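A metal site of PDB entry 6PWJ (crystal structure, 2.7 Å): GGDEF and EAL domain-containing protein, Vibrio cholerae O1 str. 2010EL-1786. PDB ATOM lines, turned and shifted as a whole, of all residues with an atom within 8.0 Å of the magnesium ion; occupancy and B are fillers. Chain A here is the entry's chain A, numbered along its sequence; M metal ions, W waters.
The side-chain carboxylate of Glu 304 sits at hydrogen-bond distance from the side-chain hydroxyl of Tyr 353, at 2.9 Å.
N of Glu 304 is in hydrogen-bond range of O of Ile 271 (2.7 Å).
The side-chain carboxylate of Glu 218 is in hydrogen-bond range of the side-chain amide nitrogen of Gln 410.
NZ of Lys 355 lies within salt-bridge range of OE1 of Glu 218 (3.4 Å).
OE2 of Glu 304 lies within salt-bridge range of NZ of Lys 355 (2.6 Å).
N of Ile 273 sits at hydrogen-bond distance from O of Glu 304 (3.0 Å).
O of Ile 305 lies within hydrogen-bond range of N of Asp 334, at 2.7 Å.
Within 4 Å of the magnesium ion: Glu 218, Asn 272, Glu 304 and Asp 334.
Along chain A the residues within 4 Å of the magnesium ion span positions 218 to 334.
OE2 of Glu 218 is bound to the magnesium ion (2.0 Å).
The magnesium ion is bound by water W1 (2.0 Å).
The magnesium ion is bound by water W2, at 2.1 Å.
OE1 of Glu 304 is bound to the magnesium ion.
OD1 of Asn 272 is bound to the magnesium ion, 2.1 Å away.
OD2 of Asp 334 binds the magnesium ion (2.1 Å).
Water W2 bridges OD1 of Asp 334 and OE1 of Glu 218.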
ATOM      1  N   HIS A 216     -12.683  30.835  26.171  1.00  0.00           N
ATOM      2  CA  HIS A 216     -13.377  29.636  25.739  1.00  0.00           C
ATOM      3  C   HIS A 216     -14.207  29.127  26.912  1.00  0.00           C
ATOM      4  O   HIS A 216     -14.215  29.728  27.998  1.00  0.00           O
ATOM      5  CB  HIS A 216     -12.409  28.569  25.208  1.00  0.00           C
ATOM      6  CG  HIS A 216     -11.490  27.990  26.247  1.00  0.00           C
ATOM      7  ND1 HIS A 216     -10.174  27.690  25.979  1.00  0.00           N
ATOM      8  CD2 HIS A 216     -11.698  27.629  27.533  1.00  0.00           C
ATOM      9  CE1 HIS A 216      -9.607  27.180  27.069  1.00  0.00           C
ATOM     10  NE2 HIS A 216     -10.519  27.136  28.018  1.00  0.00           N
ATOM     11  N   GLU A 218     -14.757  25.406  28.860  1.00  0.00           N
ATOM     12  CA  GLU A 218     -14.363  24.011  28.978  1.00  0.00           C
ATOM     13  C   GLU A 218     -15.589  23.131  29.152  1.00  0.00           C
ATOM     14  O   GLU A 218     -16.481  23.444  29.943  1.00  0.00           O
ATOM     15  CB  GLU A 218     -13.397  23.827  30.154  1.00  0.00           C
ATOM     16  CG  GLU A 218     -12.791  22.433  30.245  1.00  0.00           C
ATOM     17  CD  GLU A 218     -11.631  22.369  31.216  1.00  0.00           C
ATOM     18  OE1 GLU A 218     -11.290  23.408  31.805  1.00  0.00           O
ATOM     19  OE2 GLU A 218     -11.064  21.265  31.386  1.00  0.00           O
ATOM     20  N   VAL A 219     -15.642  22.034  28.405  1.00  0.00           N
ATOM     21  CA  VAL A 219     -16.791  21.133  28.430  1.00  0.00           C
ATOM     22  C   VAL A 219     -16.626  20.149  29.581  1.00  0.00           C
ATOM     23  O   VAL A 219     -15.542  19.580  29.780  1.00  0.00           O
ATOM     24  CB  VAL A 219     -16.933  20.405  27.090  1.00  0.00           C
ATOM     25  CG1 VAL A 219     -18.119  19.460  27.131  1.00  0.00           C
ATOM     26  CG2 VAL A 219     -17.068  21.406  25.949  1.00  0.00           C
ATOM     27  N   PHE A 220     -17.707  19.940  30.328  1.00  0.00           N
ATOM     28  CA  PHE A 220     -17.745  18.955  31.404  1.00  0.00           C
ATOM     29  C   PHE A 220     -18.956  18.062  31.195  1.00  0.00           C
ATOM     30  O   PHE A 220     -20.067  18.561  31.011  1.00  0.00           O
ATOM     31  CB  PHE A 220     -17.793  19.637  32.781  1.00  0.00           C
ATOM     32  CG  PHE A 220     -16.545  20.404  33.110  1.00  0.00           C
ATOM     33  CD1 PHE A 220     -15.467  19.783  33.707  1.00  0.00           C
ATOM     34  CD2 PHE A 220     -16.462  21.755  32.833  1.00  0.00           C
ATOM     35  CE1 PHE A 220     -14.315  20.487  34.012  1.00  0.00           C
ATOM     36  CE2 PHE A 220     -15.314  22.472  33.139  1.00  0.00           C
ATOM     37  CZ  PHE A 220     -14.244  21.833  33.732  1.00  0.00           C
ATOM     38  N   ALA A 270     -13.735  24.306  24.750  1.00  0.00           N
ATOM     39  CA  ALA A 270     -12.540  23.532  25.068  1.00  0.00           C
ATOM     40  C   ALA A 270     -12.945  22.102  25.436  1.00  0.00           C
ATOM     41  O   ALA A 270     -13.767  21.904  26.337  1.00  0.00           O
ATOM     42  CB  ALA A 270     -11.763  24.175  26.214  1.00  0.00           C
ATOM     43  N   ILE A 271     -12.385  21.129  24.733  1.00  0.00           N
ATOM     44  CA  ILE A 271     -12.659  19.720  24.961  1.00  0.00           C
ATOM     45  C   ILE A 271     -11.392  19.055  25.479  1.00  0.00           C
ATOM     46  O   ILE A 271     -10.323  19.159  24.862  1.00  0.00           O
ATOM     47  CB  ILE A 271     -13.147  19.026  23.668  1.00  0.00           C
ATOM     48  CG1 ILE A 271     -14.352  19.768  23.093  1.00  0.00           C
ATOM     49  CG2 ILE A 271     -13.486  17.578  23.946  1.00  0.00           C
ATOM     50  CD1 ILE A 271     -14.798  19.247  21.749  1.00  0.00           C
ATOM     51  N   ASN A 272     -11.500  18.389  26.628  1.00  0.00           N
ATOM     52  CA  ASN A 272     -10.380  17.656  27.192  1.00  0.00           C
ATOM     53  C   ASN A 272     -10.198  16.341  26.428  1.00  0.00           C
ATOM     54  O   ASN A 272     -11.125  15.537  26.337  1.00  0.00           O
ATOM     55  CB  ASN A 272     -10.603  17.388  28.673  1.00  0.00           C
ATOM     56  CG  ASN A 272     -10.595  18.655  29.503  1.00  0.00           C
ATOM     57  OD1 ASN A 272      -9.557  19.261  29.734  1.00  0.00           O
ATOM     58  ND2 ASN A 272     -11.776  19.056  29.976  1.00  0.00           N
ATOM     59  N   ILE A 273      -9.009  16.148  25.878  1.00  0.00           N
ATOM     60  CA  ILE A 273      -8.678  14.945  25.116  1.00  0.00           C
ATOM     61  C   ILE A 273      -7.813  14.038  25.986  1.00  0.00           C
ATOM     62  O   ILE A 273      -6.775  14.470  26.507  1.00  0.00           O
ATOM     63  CB  ILE A 273      -7.970  15.289  23.796  1.00  0.00           C
ATOM     64  CG1 ILE A 273      -8.859  16.203  22.942  1.00  0.00           C
ATOM     65  CG2 ILE A 273      -7.604  14.025  23.036  1.00  0.00           C
ATOM     66  CD1 ILE A 273     -10.181  15.577  22.549  1.00  0.00           C
ATOM     67  N   GLU A 304      -8.052  20.490  24.441  1.00  0.00           N
ATOM     68  CA  GLU A 304      -7.226  20.624  25.640  1.00  0.00           C
ATOM     69  C   GLU A 304      -6.397  19.358  25.797  1.00  0.00           C
ATOM     70  O   GLU A 304      -6.919  18.315  26.193  1.00  0.00           O
ATOM     71  CB  GLU A 304      -8.097  20.886  26.868  1.00  0.00           C
ATOM     72  CG  GLU A 304      -7.423  21.720  27.937  1.00  0.00           C
ATOM     73  CD  GLU A 304      -8.419  22.497  28.779  1.00  0.00           C
ATOM     74  OE1 GLU A 304      -8.925  21.950  29.774  1.00  0.00           O
ATOM     75  OE2 GLU A 304      -8.700  23.662  28.423  1.00  0.00           O
ATOM     76  N   ILE A 305      -5.108  19.462  25.500  1.00  0.00           N
ATOM     77  CA  ILE A 305      -4.190  18.329  25.552  1.00  0.00           C
ATOM     78  C   ILE A 305      -3.466  18.362  26.888  1.00  0.00           C
ATOM     79  O   ILE A 305      -2.881  19.405  27.240  1.00  0.00           O
ATOM     80  CB  ILE A 305      -3.189  18.351  24.394  1.00  0.00           C
ATOM     81  CG1 ILE A 305      -3.887  18.716  23.084  1.00  0.00           C
ATOM     82  CG2 ILE A 305      -2.480  17.007  24.270  1.00  0.00           C
ATOM     83  CD1 ILE A 305      -4.965  17.734  22.670  1.00  0.00           C
ATOM     84  N   PRO A 306      -3.473  17.277  27.677  1.00  0.00           N
ATOM     85  CA  PRO A 306      -2.658  17.256  28.885  1.00  0.00           C
ATOM     86  C   PRO A 306      -1.184  17.419  28.551  1.00  0.00           C
ATOM     87  O   PRO A 306      -0.732  17.103  27.454  1.00  0.00           O
ATOM     88  CB  PRO A 306      -2.943  15.862  29.478  1.00  0.00           C
ATOM     89  CG  PRO A 306      -4.267  15.473  28.905  1.00  0.00           C
ATOM     90  CD  PRO A 306      -4.308  16.072  27.530  1.00  0.00           C
ATOM     91  N   VAL A 333      -2.604  23.539  26.261  1.00  0.00           N
ATOM     92  CA  VAL A 333      -1.967  22.638  27.205  1.00  0.00           C
ATOM     93  C   VAL A 333      -2.752  22.651  28.508  1.00  0.00           C
ATOM     94  O   VAL A 333      -2.948  23.718  29.112  1.00  0.00           O
ATOM     95  CB  VAL A 333      -0.496  23.022  27.441  1.00  0.00           C
ATOM     96  CG1 VAL A 333       0.171  22.027  28.392  1.00  0.00           C
ATOM     97  CG2 VAL A 333       0.257  23.096  26.120  1.00  0.00           C
ATOM     98  N   ASP A 334      -3.196  21.483  28.940  1.00  0.00           N
ATOM     99  CA  ASP A 334      -3.891  21.325  30.215  1.00  0.00           C
ATOM    100  C   ASP A 334      -2.918  20.758  31.240  1.00  0.00           C
ATOM    101  O   ASP A 334      -2.119  19.872  30.926  1.00  0.00           O
ATOM    102  CB  ASP A 334      -5.111  20.420  30.075  1.00  0.00           C
ATOM    103  CG  ASP A 334      -6.146  20.659  31.152  1.00  0.00           C
ATOM    104  OD1 ASP A 334      -5.912  21.516  32.032  1.00  0.00           O
ATOM    105  OD2 ASP A 334      -7.212  20.006  31.116  1.00  0.00           O
ATOM    106  N   ASN A 335      -2.980  21.283  32.458  1.00  0.00           N
ATOM    107  CA  ASN A 335      -2.058  20.877  33.521  1.00  0.00           C
ATOM    108  C   ASN A 335      -0.624  21.296  33.187  1.00  0.00           C
ATOM    109  O   ASN A 335       0.332  20.567  33.446  1.00  0.00           O
ATOM    110  CB  ASN A 335      -2.137  19.371  33.778  1.00  0.00           C
ATOM    111  CG  ASN A 335      -3.535  18.913  34.116  1.00  0.00           C
ATOM    112  OD1 ASN A 335      -4.205  19.490  34.979  1.00  0.00           O
ATOM    113  ND2 ASN A 335      -4.012  17.881  33.430  1.00  0.00           N
ATOM    114  N   TYR A 353      -2.949  28.209  24.140  1.00  0.00           N
ATOM    115  CA  TYR A 353      -3.055  28.586  25.536  1.00  0.00           C
ATOM    116  C   TYR A 353      -2.414  27.502  26.395  1.00  0.00           C
ATOM    117  O   TYR A 353      -2.204  26.367  25.944  1.00  0.00           O
ATOM    118  CB  TYR A 353      -4.520  28.791  25.960  1.00  0.00           C
ATOM    119  CG  TYR A 353      -5.364  27.535  25.898  1.00  0.00           C
ATOM    120  CD1 TYR A 353      -5.373  26.614  26.937  1.00  0.00           C
ATOM    121  CD2 TYR A 353      -6.170  27.278  24.793  1.00  0.00           C
ATOM    122  CE1 TYR A 353      -6.148  25.473  26.877  1.00  0.00           C
ATOM    123  CE2 TYR A 353      -6.951  26.143  24.721  1.00  0.00           C
ATOM    124  CZ  TYR A 353      -6.931  25.239  25.771  1.00  0.00           C
ATOM    125  OH  TYR A 353      -7.703  24.099  25.701  1.00  0.00           O
ATOM    126  N   LYS A 355      -3.116  25.932  30.265  1.00  0.00           N
ATOM    127  CA  LYS A 355      -3.927  25.885  31.491  1.00  0.00           C
ATOM    128  C   LYS A 355      -3.013  25.422  32.617  1.00  0.00           C
ATOM    129  O   LYS A 355      -2.718  24.239  32.745  1.00  0.00           O
ATOM    130  CB  LYS A 355      -5.121  24.952  31.323  1.00  0.00           C
ATOM    131  CG  LYS A 355      -6.456  25.657  31.178  1.00  0.00           C
ATOM    132  CD  LYS A 355      -7.588  24.770  31.658  1.00  0.00           C
ATOM    133  CE  LYS A 355      -8.943  25.436  31.524  1.00  0.00           C
ATOM    134  NZ  LYS A 355      -9.350  25.541  30.092  1.00  0.00           N
ATOM    135  N   SER A 390      -7.295  27.902  36.243  1.00  0.00           N
ATOM    136  CA  SER A 390      -8.617  27.339  36.453  1.00  0.00           C
ATOM    137  C   SER A 390      -8.854  27.089  37.933  1.00  0.00           C
ATOM    138  O   SER A 390      -7.964  27.249  38.777  1.00  0.00           O
ATOM    139  CB  SER A 390      -8.782  26.031  35.669  1.00  0.00           C
ATOM    140  OG  SER A 390      -8.129  24.950  36.313  1.00  0.00           O
ATOM    141  N   GLN A 410     -10.889  30.918  35.282  1.00  0.00           N
ATOM    142  CA  GLN A 410     -11.983  29.965  35.190  1.00  0.00           C
ATOM    143  C   GLN A 410     -12.249  29.393  36.569  1.00  0.00           C
ATOM    144  O   GLN A 410     -11.316  29.084  37.314  1.00  0.00           O
ATOM    145  CB  GLN A 410     -11.647  28.840  34.200  1.00  0.00           C
ATOM    146  CG  GLN A 410     -12.683  27.734  34.115  1.00  0.00           C
ATOM    147  CD  GLN A 410     -12.299  26.672  33.103  1.00  0.00           C
ATOM    148  OE1 GLN A 410     -11.403  26.871  32.285  1.00  0.00           O
ATOM    149  NE2 GLN A 410     -12.968  25.519  33.164  1.00  0.00           N
HETATM  150 MG    MG M   1      -9.215  20.578  31.286  1.00  0.00          MG
HETATM  151  O   HOH W   1      -9.263  19.671  33.109  1.00  0.00           O
HETATM  152  O   HOH W   2      -8.416  21.789  32.739  1.00  0.00           O
